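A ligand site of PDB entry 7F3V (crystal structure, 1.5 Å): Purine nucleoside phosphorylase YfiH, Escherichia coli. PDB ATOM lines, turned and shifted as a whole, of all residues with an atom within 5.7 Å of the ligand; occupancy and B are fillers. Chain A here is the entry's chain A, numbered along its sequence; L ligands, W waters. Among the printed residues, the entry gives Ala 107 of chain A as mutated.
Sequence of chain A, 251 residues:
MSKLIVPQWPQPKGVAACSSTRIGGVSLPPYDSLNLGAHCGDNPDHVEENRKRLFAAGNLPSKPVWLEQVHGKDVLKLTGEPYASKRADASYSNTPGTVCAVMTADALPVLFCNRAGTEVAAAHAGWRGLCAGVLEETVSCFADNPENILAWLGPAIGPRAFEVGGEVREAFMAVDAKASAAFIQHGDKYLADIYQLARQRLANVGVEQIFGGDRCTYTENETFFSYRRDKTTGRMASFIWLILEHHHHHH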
ATOM      1  N   GLN A  69      16.018 -21.975  36.430  1.00  0.00           N
ATOM      2  CA  GLN A  69      15.278 -22.492  35.260  1.00  0.00           C
ATOM      3  C   GLN A  69      15.980 -22.116  33.971  1.00  0.00           C
ATOM      4  O   GLN A  69      16.333 -20.945  33.801  1.00  0.00           O
ATOM      5  CB  GLN A  69      13.850 -21.951  35.304  1.00  0.00           C
ATOM      6  CG  GLN A  69      13.104 -22.436  36.533  1.00  0.00           C
ATOM      7  CD  GLN A  69      11.667 -22.006  36.662  1.00  0.00           C
ATOM      8  OE1 GLN A  69      11.009 -22.306  37.682  1.00  0.00           O
ATOM      9  NE2 GLN A  69      11.132 -21.317  35.639  1.00  0.00           N
ATOM     10  N   HIS A  71      14.805 -23.704  30.782  1.00  0.00           N
ATOM     11  CA  HIS A  71      13.943 -24.242  29.683  1.00  0.00           C
ATOM     12  C   HIS A  71      14.467 -25.602  29.204  1.00  0.00           C
ATOM     13  O   HIS A  71      14.415 -25.903  28.021  1.00  0.00           O
ATOM     14  CB  HIS A  71      13.727 -23.206  28.559  1.00  0.00           C
ATOM     15  CG  HIS A  71      12.863 -22.080  29.041  1.00  0.00           C
ATOM     16  ND1 HIS A  71      11.494 -22.071  28.783  1.00  0.00           N
ATOM     17  CD2 HIS A  71      13.148 -20.923  29.726  1.00  0.00           C
ATOM     18  CE1 HIS A  71      10.958 -20.994  29.312  1.00  0.00           C
ATOM     19  NE2 HIS A  71      11.980 -20.265  29.904  1.00  0.00           N
ATOM     20  N   MET A 103       8.374 -21.233  38.291  1.00  0.00           N
ATOM     21  CA  MET A 103       8.056 -19.816  38.021  1.00  0.00           C
ATOM     22  C   MET A 103       7.690 -19.690  36.549  1.00  0.00           C
ATOM     23  O   MET A 103       8.385 -20.266  35.736  1.00  0.00           O
ATOM     24  CB  MET A 103       9.240 -18.867  38.310  1.00  0.00           C
ATOM     25  CG  MET A 103       9.389 -18.640  39.782  1.00  0.00           C
ATOM     26  SD  MET A 103      10.883 -17.641  40.113  1.00  0.00           S
ATOM     27  CE  MET A 103      12.147 -18.819  39.668  1.00  0.00           C
ATOM     28  N   THR A 104       6.568 -19.045  36.261  1.00  0.00           N
ATOM     29  CA  THR A 104       5.999 -18.977  34.894  1.00  0.00           C
ATOM     30  C   THR A 104       5.326 -17.634  34.595  1.00  0.00           C
ATOM     31  O   THR A 104       4.844 -16.977  35.529  1.00  0.00           O
ATOM     32  CB  THR A 104       4.991 -20.118  34.650  1.00  0.00           C
ATOM     33  OG1 THR A 104       3.753 -19.819  35.271  1.00  0.00           O
ATOM     34  CG2 THR A 104       5.531 -21.448  35.143  1.00  0.00           C
ATOM     35  N   ALA A 105       5.249 -17.317  33.303  1.00  0.00           N
ATOM     36  CA  ALA A 105       4.427 -16.213  32.746  1.00  0.00           C
ATOM     37  C   ALA A 105       4.147 -16.549  31.294  1.00  0.00           C
ATOM     38  O   ALA A 105       4.519 -15.791  30.427  1.00  0.00           O
ATOM     39  CB  ALA A 105       5.145 -14.873  32.875  1.00  0.00           C
ATOM     40  N   ASP A 106       3.523 -17.701  31.088  1.00  0.00           N
ATOM     41  CA  ASP A 106       3.013 -18.276  29.810  1.00  0.00           C
ATOM     42  C   ASP A 106       3.393 -19.767  29.718  1.00  0.00           C
ATOM     43  O   ASP A 106       2.601 -20.572  29.194  1.00  0.00           O
ATOM     44  CB  ASP A 106       3.541 -17.610  28.548  1.00  0.00           C
ATOM     45  CG  ASP A 106       2.929 -16.257  28.205  1.00  0.00           C
ATOM     46  OD1 ASP A 106       1.856 -15.909  28.757  1.00  0.00           O
ATOM     47  OD2 ASP A 106       3.595 -15.589  27.362  1.00  0.00           O
ATOM     48  N   ALA A 107       4.594 -20.113  30.168  1.00  0.00           N
ATOM     49  CA  ALA A 107       5.004 -21.541  30.147  1.00  0.00           C
ATOM     50  C   ALA A 107       4.029 -22.339  30.998  1.00  0.00           C
ATOM     51  O   ALA A 107       3.533 -21.853  31.991  1.00  0.00           O
ATOM     52  CB  ALA A 107       6.401 -21.722  30.669  1.00  0.00           C
ATOM     53  N   LEU A 108       3.821 -23.590  30.631  1.00  0.00           N
ATOM     54  CA  LEU A 108       2.882 -24.433  31.378  1.00  0.00           C
ATOM     55  C   LEU A 108       3.507 -24.895  32.685  1.00  0.00           C
ATOM     56  O   LEU A 108       4.502 -25.626  32.650  1.00  0.00           O
ATOM     57  CB  LEU A 108       2.541 -25.622  30.497  1.00  0.00           C
ATOM     58  CG  LEU A 108       1.635 -26.682  31.105  1.00  0.00           C
ATOM     59  CD1 LEU A 108       0.233 -26.158  31.426  1.00  0.00           C
ATOM     60  CD2 LEU A 108       1.634 -27.899  30.179  1.00  0.00           C
ATOM     61  N   HIS A 124       8.215 -26.924  35.031  1.00  0.00           N
ATOM     62  CA  HIS A 124       8.186 -25.714  34.166  1.00  0.00           C
ATOM     63  C   HIS A 124       8.289 -26.153  32.721  1.00  0.00           C
ATOM     64  O   HIS A 124       9.344 -26.471  32.297  1.00  0.00           O
ATOM     65  CB  HIS A 124       9.349 -24.804  34.554  1.00  0.00           C
ATOM     66  CG  HIS A 124       9.593 -23.642  33.624  1.00  0.00           C
ATOM     67  ND1 HIS A 124      10.809 -23.486  32.980  1.00  0.00           N
ATOM     68  CD2 HIS A 124       8.823 -22.567  33.292  1.00  0.00           C
ATOM     69  CE1 HIS A 124      10.764 -22.363  32.249  1.00  0.00           C
ATOM     70  NE2 HIS A 124       9.552 -21.820  32.380  1.00  0.00           N
ATOM     71  N   ALA A 125       7.148 -26.213  32.030  1.00  0.00           N
ATOM     72  CA  ALA A 125       7.064 -26.703  30.660  1.00  0.00           C
ATOM     73  C   ALA A 125       6.764 -25.562  29.674  1.00  0.00           C
ATOM     74  O   ALA A 125       5.638 -25.430  29.171  1.00  0.00           O
ATOM     75  CB  ALA A 125       6.051 -27.820  30.572  1.00  0.00           C
ATOM     76  N   GLY A 126       7.755 -24.705  29.455  1.00  0.00           N
ATOM     77  CA  GLY A 126       7.693 -23.849  28.274  1.00  0.00           C
ATOM     78  C   GLY A 126       7.764 -24.712  27.027  1.00  0.00           C
ATOM     79  O   GLY A 126       8.000 -25.925  27.125  1.00  0.00           O
ATOM     80  N   TRP A 127       7.635 -24.135  25.838  1.00  0.00           N
ATOM     81  CA  TRP A 127       7.636 -24.985  24.630  1.00  0.00           C
ATOM     82  C   TRP A 127       8.949 -25.745  24.557  1.00  0.00           C
ATOM     83  O   TRP A 127       8.939 -26.927  24.161  1.00  0.00           O
ATOM     84  CB  TRP A 127       7.336 -24.138  23.382  1.00  0.00           C
ATOM     85  CG  TRP A 127       8.377 -23.172  22.931  1.00  0.00           C
ATOM     86  CD1 TRP A 127       8.338 -21.811  23.081  1.00  0.00           C
ATOM     87  CD2 TRP A 127       9.529 -23.486  22.130  1.00  0.00           C
ATOM     88  NE1 TRP A 127       9.455 -21.268  22.496  1.00  0.00           N
ATOM     89  CE2 TRP A 127      10.187 -22.253  21.885  1.00  0.00           C
ATOM     90  CE3 TRP A 127      10.058 -24.676  21.615  1.00  0.00           C
ATOM     91  CZ2 TRP A 127      11.376 -22.186  21.151  1.00  0.00           C
ATOM     92  CZ3 TRP A 127      11.231 -24.610  20.896  1.00  0.00           C
ATOM     93  CH2 TRP A 127      11.872 -23.379  20.666  1.00  0.00           C
ATOM     94  N   ARG A 128      10.086 -25.129  24.899  1.00  0.00           N
ATOM     95  CA  ARG A 128      11.405 -25.764  24.649  1.00  0.00           C
ATOM     96  C   ARG A 128      11.579 -26.957  25.586  1.00  0.00           C
ATOM     97  O   ARG A 128      12.019 -28.019  25.120  1.00  0.00           O
ATOM     98  CB  ARG A 128      12.587 -24.782  24.806  1.00  0.00           C
ATOM     99  CG  ARG A 128      12.654 -23.695  23.750  1.00  0.00           C
ATOM    100  CD  ARG A 128      13.933 -22.851  23.754  1.00  0.00           C
ATOM    101  NE  ARG A 128      13.775 -21.528  23.178  1.00  0.00           N
ATOM    102  CZ  ARG A 128      13.087 -20.582  23.787  1.00  0.00           C
ATOM    103  NH1 ARG A 128      12.614 -20.966  24.958  1.00  0.00           N
ATOM    104  NH2 ARG A 128      12.956 -19.318  23.293  1.00  0.00           N
ATOM    105  N   ILE A 157      -0.126 -20.074  28.437  1.00  0.00           N
ATOM    106  CA  ILE A 157      -0.619 -19.356  27.225  1.00  0.00           C
ATOM    107  C   ILE A 157      -1.394 -20.379  26.388  1.00  0.00           C
ATOM    108  O   ILE A 157      -0.813 -21.359  25.891  1.00  0.00           O
ATOM    109  CB  ILE A 157       0.513 -18.618  26.499  1.00  0.00           C
ATOM    110  CG1 ILE A 157      -0.048 -17.795  25.356  1.00  0.00           C
ATOM    111  CG2 ILE A 157       1.589 -19.544  25.995  1.00  0.00           C
ATOM    112  CD1 ILE A 157       0.937 -16.837  24.710  1.00  0.00           C
ATOM    113  N   PHE A 162      -1.143 -18.437  21.557  1.00  0.00           N
ATOM    114  CA  PHE A 162       0.232 -18.961  21.452  1.00  0.00           C
ATOM    115  C   PHE A 162       0.605 -19.109  19.991  1.00  0.00           C
ATOM    116  O   PHE A 162       0.705 -20.215  19.470  1.00  0.00           O
ATOM    117  CB  PHE A 162       0.393 -20.215  22.302  1.00  0.00           C
ATOM    118  CG  PHE A 162       1.812 -20.678  22.474  1.00  0.00           C
ATOM    119  CD1 PHE A 162       2.902 -19.795  22.423  1.00  0.00           C
ATOM    120  CD2 PHE A 162       2.083 -22.018  22.656  1.00  0.00           C
ATOM    121  CE1 PHE A 162       4.188 -20.254  22.624  1.00  0.00           C
ATOM    122  CE2 PHE A 162       3.373 -22.475  22.880  1.00  0.00           C
ATOM    123  CZ  PHE A 162       4.423 -21.594  22.853  1.00  0.00           C
ATOM    124  N   GLU A 163       0.912 -18.001  19.328  1.00  0.00           N
ATOM    125  CA  GLU A 163       1.355 -18.014  17.944  1.00  0.00           C
ATOM    126  C   GLU A 163       2.826 -18.424  17.907  1.00  0.00           C
ATOM    127  O   GLU A 163       3.655 -17.881  18.641  1.00  0.00           O
ATOM    128  CB  GLU A 163       1.083 -16.656  17.341  1.00  0.00           C
ATOM    129  CG  GLU A 163       1.510 -16.602  15.894  1.00  0.00           C
ATOM    130  CD  GLU A 163       1.380 -15.217  15.282  1.00  0.00           C
ATOM    131  OE1 GLU A 163       0.759 -15.123  14.211  1.00  0.00           O
ATOM    132  OE2 GLU A 163       1.965 -14.245  15.843  1.00  0.00           O
ATOM    133  N   VAL A 164       3.161 -19.412  17.091  1.00  0.00           N
ATOM    134  CA  VAL A 164       4.567 -19.871  16.920  1.00  0.00           C
ATOM    135  C   VAL A 164       4.884 -20.052  15.455  1.00  0.00           C
ATOM    136  O   VAL A 164       3.925 -20.145  14.660  1.00  0.00           O
ATOM    137  CB  VAL A 164       4.837 -21.159  17.707  1.00  0.00           C
ATOM    138  CG1 VAL A 164       4.506 -20.933  19.162  1.00  0.00           C
ATOM    139  CG2 VAL A 164       4.081 -22.361  17.116  1.00  0.00           C
ATOM    140  N   GLY A 165       6.174 -20.038  15.102  1.00  0.00           N
ATOM    141  CA  GLY A 165       6.692 -20.409  13.781  1.00  0.00           C
ATOM    142  C   GLY A 165       7.291 -21.809  13.736  1.00  0.00           C
ATOM    143  O   GLY A 165       7.010 -22.591  14.666  1.00  0.00           O
ATOM    144  N   GLY A 166       8.172 -22.112  12.763  1.00  0.00           N
ATOM    145  CA  GLY A 166       8.883 -23.400  12.594  1.00  0.00           C
ATOM    146  C   GLY A 166       9.946 -23.704  13.625  1.00  0.00           C
ATOM    147  O   GLY A 166      10.198 -24.889  13.888  1.00  0.00           O
ATOM    148  N   GLU A 167      10.581 -22.705  14.250  1.00  0.00           N
ATOM    149  CA  GLU A 167      11.525 -22.995  15.352  1.00  0.00           C
ATOM    150  C   GLU A 167      10.827 -24.053  16.232  1.00  0.00           C
ATOM    151  O   GLU A 167      11.419 -25.101  16.526  1.00  0.00           O
ATOM    152  CB  GLU A 167      11.901 -21.715  16.109  1.00  0.00           C
ATOM    153  CG  GLU A 167      13.250 -21.799  16.819  1.00  0.00           C
ATOM    154  CD  GLU A 167      13.391 -20.906  18.034  1.00  0.00           C
ATOM    155  OE1 GLU A 167      12.643 -19.919  18.140  1.00  0.00           O
ATOM    156  OE2 GLU A 167      14.241 -21.234  18.893  1.00  0.00           O
ATOM    157  N   VAL A 168       9.549 -23.846  16.516  1.00  0.00           N
ATOM    158  CA  VAL A 168       8.753 -24.657  17.486  1.00  0.00           C
ATOM    159  C   VAL A 168       8.129 -25.886  16.811  1.00  0.00           C
ATOM    160  O   VAL A 168       8.222 -26.988  17.404  1.00  0.00           O
ATOM    161  CB  VAL A 168       7.675 -23.801  18.152  1.00  0.00           C
ATOM    162  CG1 VAL A 168       6.963 -24.571  19.237  1.00  0.00           C
ATOM    163  CG2 VAL A 168       8.286 -22.548  18.730  1.00  0.00           C
ATOM    164  N   LYS A 189       1.988 -18.245  10.372  1.00  0.00           N
ATOM    165  CA  LYS A 189       2.460 -18.894  11.621  1.00  0.00           C
ATOM    166  C   LYS A 189       1.471 -20.001  11.989  1.00  0.00           C
ATOM    167  O   LYS A 189       0.697 -20.426  11.141  1.00  0.00           O
ATOM    168  CB  LYS A 189       2.648 -17.833  12.705  1.00  0.00           C
ATOM    169  CG  LYS A 189       3.843 -16.928  12.407  1.00  0.00           C
ATOM    170  CD  LYS A 189       3.947 -15.705  13.279  1.00  0.00           C
ATOM    171  CE  LYS A 189       5.276 -14.991  13.120  1.00  0.00           C
ATOM    172  NZ  LYS A 189       6.412 -15.930  12.970  1.00  0.00           N
ATOM    173  N   ILE A 194      -0.586 -25.777  23.898  1.00  0.00           N
ATOM    174  CA  ILE A 194       0.407 -26.288  24.860  1.00  0.00           C
ATOM    175  C   ILE A 194      -0.244 -27.321  25.779  1.00  0.00           C
ATOM    176  O   ILE A 194       0.461 -28.232  26.236  1.00  0.00           O
ATOM    177  CB  ILE A 194       1.043 -25.101  25.617  1.00  0.00           C
ATOM    178  CG1 ILE A 194       2.411 -25.499  26.210  1.00  0.00           C
ATOM    179  CG2 ILE A 194       0.123 -24.545  26.667  1.00  0.00           C
ATOM    180  CD1 ILE A 194       3.159 -24.274  26.742  1.00  0.00           C
ATOM    181  N   TYR A 227       4.464 -13.101  29.311  1.00  0.00           N
ATOM    182  CA  TYR A 227       5.632 -12.618  28.538  1.00  0.00           C
ATOM    183  C   TYR A 227       5.164 -12.209  27.150  1.00  0.00           C
ATOM    184  O   TYR A 227       5.605 -11.173  26.591  1.00  0.00           O
ATOM    185  CB  TYR A 227       6.707 -13.685  28.520  1.00  0.00           C
ATOM    186  CG  TYR A 227       7.807 -13.413  27.552  1.00  0.00           C
ATOM    187  CD1 TYR A 227       8.545 -12.222  27.640  1.00  0.00           C
ATOM    188  CD2 TYR A 227       8.125 -14.260  26.527  1.00  0.00           C
ATOM    189  CE1 TYR A 227       9.542 -11.929  26.715  1.00  0.00           C
ATOM    190  CE2 TYR A 227       9.136 -13.996  25.628  1.00  0.00           C
ATOM    191  CZ  TYR A 227       9.831 -12.827  25.701  1.00  0.00           C
ATOM    192  OH  TYR A 227      10.824 -12.639  24.800  1.00  0.00           O
ATOM    193  N   ARG A 228       4.358 -13.053  26.488  1.00  0.00           N
ATOM    194  CA  ARG A 228       3.933 -12.770  25.107  1.00  0.00           C
ATOM    195  C   ARG A 228       3.102 -11.472  25.062  1.00  0.00           C
ATOM    196  O   ARG A 228       3.309 -10.690  24.119  1.00  0.00           O
ATOM    197  CB  ARG A 228       3.109 -13.918  24.541  1.00  0.00           C
ATOM    198  CG  ARG A 228       2.826 -13.739  23.051  1.00  0.00           C
ATOM    199  CD  ARG A 228       4.072 -13.746  22.193  1.00  0.00           C
ATOM    200  NE  ARG A 228       4.708 -15.059  22.091  1.00  0.00           N
ATOM    201  CZ  ARG A 228       4.392 -15.971  21.187  1.00  0.00           C
ATOM    202  NH1 ARG A 228       3.372 -15.738  20.386  1.00  0.00           N
ATOM    203  NH2 ARG A 228       5.061 -17.089  21.121  1.00  0.00           N
ATOM    204  N   ARG A 235       6.495 -12.629  37.055  1.00  0.00           N
ATOM    205  CA  ARG A 235       6.367 -14.122  37.054  1.00  0.00           C
ATOM    206  C   ARG A 235       5.426 -14.514  38.181  1.00  0.00           C
ATOM    207  O   ARG A 235       5.539 -13.995  39.294  1.00  0.00           O
ATOM    208  CB  ARG A 235       7.699 -14.829  37.225  1.00  0.00           C
ATOM    209  CG  ARG A 235       8.710 -14.519  36.138  1.00  0.00           C
ATOM    210  CD  ARG A 235       8.401 -15.077  34.769  1.00  0.00           C
ATOM    211  NE  ARG A 235       9.457 -14.772  33.817  1.00  0.00           N
ATOM    212  CZ  ARG A 235       9.503 -13.736  33.023  1.00  0.00           C
ATOM    213  NH1 ARG A 235       8.540 -12.843  33.064  1.00  0.00           N
ATOM    214  NH2 ARG A 235      10.552 -13.535  32.250  1.00  0.00           N
HETATM  215  C1  LIG L   1       9.373 -18.491  25.222  1.00  0.00           C
HETATM  216  O1  LIG L   1       8.643 -17.333  24.869  1.00  0.00           O
HETATM  217  C2  LIG L   1       8.904 -18.923  26.619  1.00  0.00           C
HETATM  218  N1  LIG L   1       7.482 -19.123  26.605  1.00  0.00           N
HETATM  219  C3  LIG L   1       9.357 -17.921  27.686  1.00  0.00           C
HETATM  220  O2  LIG L   1       9.152 -18.430  28.997  1.00  0.00           O
HETATM  221  C4  LIG L   1      10.843 -17.705  27.559  1.00  0.00           C
HETATM  222  O3  LIG L   1      11.240 -16.717  28.500  1.00  0.00           O
HETATM  223  C5  LIG L   1      11.218 -17.283  26.153  1.00  0.00           C
HETATM  224  O4  LIG L   1      10.767 -18.261  25.195  1.00  0.00           O
HETATM  225  C6  LIG L   1      12.746 -17.272  26.031  1.00  0.00           C
HETATM  226  O5  LIG L   1      13.123 -16.787  24.804  1.00  0.00           O
HETATM  227  C7  LIG L   1       6.928 -20.352  26.480  1.00  0.00           C
HETATM  228  O6  LIG L   1       7.622 -21.336  26.370  1.00  0.00           O
HETATM  229  C8  LIG L   1       5.446 -20.410  26.352  1.00  0.00           C
HETATM  230  P1  LIG L   1      10.044 -17.351  21.569  1.00  0.00           P
HETATM  231  P2  LIG L   1       7.855 -17.192  23.478  1.00  0.00           P
HETATM  232  O7  LIG L   1      10.537 -18.610  22.178  1.00  0.00           O
HETATM  233  O8  LIG L   1       7.401 -18.517  22.995  1.00  0.00           O
HETATM  234  C9  LIG L   1       7.097 -17.187  17.417  1.00  0.00           C
HETATM  235  C10 LIG L   1       7.874 -18.757  30.975  1.00  0.00           C
HETATM  236  O9  LIG L   1       6.726 -18.768  31.509  1.00  0.00           O
HETATM  237  N2  LIG L   1       6.443 -15.934  17.724  1.00  0.00           N
HETATM  238  O10 LIG L   1      11.048 -16.295  21.225  1.00  0.00           O
HETATM  239  O11 LIG L   1       6.916 -16.077  23.673  1.00  0.00           O
HETATM  240  C11 LIG L   1       8.606 -17.111  17.207  1.00  0.00           C
HETATM  241  O12 LIG L   1       8.859 -16.689  15.874  1.00  0.00           O
HETATM  242  C12 LIG L   1       8.029 -17.958  29.726  1.00  0.00           C
HETATM  243  O13 LIG L   1       8.907 -19.331  31.419  1.00  0.00           O
HETATM  244  C13 LIG L   1       5.366 -15.569  16.941  1.00  0.00           C
HETATM  245  O14 LIG L   1       4.948 -16.249  16.022  1.00  0.00           O
HETATM  246  O15 LIG L   1       8.981 -16.650  22.500  1.00  0.00           O
HETATM  247  C14 LIG L   1       8.982 -18.579  17.462  1.00  0.00           C
HETATM  248  O16 LIG L   1       8.689 -19.456  16.389  1.00  0.00           O
HETATM  249  C15 LIG L   1       8.181 -16.505  30.140  1.00  0.00           C
HETATM  250  N3  LIG L   1       4.750 -14.435  17.342  1.00  0.00           N
HETATM  251  C16 LIG L   1       8.024 -18.934  18.621  1.00  0.00           C
HETATM  252  O17 LIG L   1       6.921 -17.996  18.563  1.00  0.00           O
HETATM  253  C17 LIG L   1       5.106 -13.588  18.355  1.00  0.00           C
HETATM  254  O18 LIG L   1       4.424 -12.590  18.579  1.00  0.00           O
HETATM  255  C18 LIG L   1       8.641 -18.930  20.002  1.00  0.00           C
HETATM  256  O19 LIG L   1       9.247 -17.610  20.179  1.00  0.00           O
HETATM  257  C19 LIG L   1       6.237 -14.018  19.125  1.00  0.00           C
HETATM  258  C20 LIG L   1       6.842 -15.162  18.789  1.00  0.00           C
HETATM  259  O   HOH W   1       5.011 -10.626  19.832  1.00  0.00           O
HETATM  260  O   HOH W   2       7.524 -13.537  22.751  1.00  0.00           O
HETATM  261  O   HOH W   3      11.880 -14.770  23.431  1.00  0.00           O
HETATM  262  O   HOH W   4       1.459 -13.625  19.777  1.00  0.00           O
HETATM  263  O   HOH W   5       9.855 -18.234  34.108  1.00  0.00           O
HETATM  264  O   HOH W   6      10.391 -19.870  14.264  1.00  0.00           O
HETATM  265  O   HOH W   7      15.778 -16.366  24.899  1.00  0.00           O
HETATM  266  O   HOH W   8      10.393 -22.321  26.063  1.00  0.00           O
HETATM  267  O   HOH W   9       9.508 -13.796  20.960  1.00  0.00           O
HETATM  268  O   HOH W  10      13.916 -16.911  29.610  1.00  0.00           O
HETATM  269  O   HOH W  11       5.745 -16.856  26.210  1.00  0.00           O
HETATM  270  O   HOH W  12      13.618 -16.613  20.690  1.00  0.00           O
HETATM  271  O   HOH W  13      11.251 -17.741  31.100  1.00  0.00           O
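NE2 of His 124 lies within hydrogen-bond range of O13 of the ligand, 2.7 Å away. N of Ala 105 lies within hydrogen-bond range of O9 of the ligand, at 2.7 Å. The guanidinium group (NE) of Arg 228 lies within salt-bridge range of an oxygen (O11) of the ligand (2.9 Å). A ring nitrogen (NE2) of His 71 lies close to an oxygen (O2) of the ligand (3.5 Å). The backbone NH (N) of Gly 165 lies within hydrogen-bond range of an oxygen (O16) of the ligand. An oxygen (O6) of the ligand is in hydrogen-bond range of the backbone NH (N) of Trp 127 (2.8 Å). An oxygen (O9) of the ligand lies within hydrogen-bond range of the backbone NH of Ala 107, at 2.9 Å. An oxygen (O7) of the ligand sits at hydrogen-bond distance from the indole nitrogen of Trp 127, 2.9 Å away. N of Asp 106 sits at hydrogen-bond distance from O9 of the ligand (3.4 Å). The side-chain amino group (NZ) of Lys 189 lies close to an oxygen (O14) of the ligand (3.4 Å). NH2 of Arg 128 lies within salt-bridge range of O7 of the ligand (2.8 Å). The side-chain carboxylate (OE2) of Glu 163 is in hydrogen-bond range of a nitrogen (N3) of the ligand (3.2 Å).
Water W3 bridges an oxygen (O5) of the ligand (2.7 Å) and the side-chain hydroxyl of Tyr 227 (2.7 Å). Water W6 lies within hydrogen-bond range of an oxygen (O16) of the ligand, the backbone NH (N) of Glu 167 and the backbone NH (N) of Gly 166. Water W2 lies within hydrogen-bond range of O11 of the ligand (2.8 Å) and NE of Arg 228 (3.3 Å). Water W13 bridges an oxygen (O3) of the ligand (2.8 Å) and a ring nitrogen (NE2) of His 71 (2.9 Å). Water W11 bridges OD2 of Asp 106 (2.7 Å) and N1 of the ligand (2.9 Å). Water W5 lies within hydrogen-bond range of the backbone carbonyl oxygen of Met 103 (3.0 Å), an oxygen (O13) of the ligand (3.1 Å) and the guanidinium group of Arg 235 (3.5 Å).
ND1 of His 124 sits close to NE2 of Gln 69 (3.4 Å). The side-chain carboxylate of Asp 106 lies within hydrogen-bond range of the backbone NH of Arg 228, 2.8 Å away. The side-chain carboxylate of Asp 106 is in hydrogen-bond range of the backbone NH of Tyr 227. O of Asp 106 lies within hydrogen-bond range of N of Ile 157 (2.9 Å). NH1 of Arg 228 is in hydrogen-bond range of O of Glu 163, at 2.8 Å. O of Ala 105 is in hydrogen-bond range of N of Tyr 227.
Merely in contact with the ligand: Gly 126 (3.2 Å), Val 164 (3.4 Å), Tyr 227 (3.5 Å), Thr 104 (3.5 Å), Val 168 (3.6 Å), Phe 162 (3.7 Å), Glu 167 (3.9 Å) and Ile 157 (3.97 Å). Hydrophobic or aromatic side chains within 4 Å of the ligand: His 71, Ala 107, His 124, Trp 127, Ile 157, Phe 162, Val 164, Val 168 and Tyr 227. Of the 26 residues printed, 19 come within 4 Å of the ligand.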
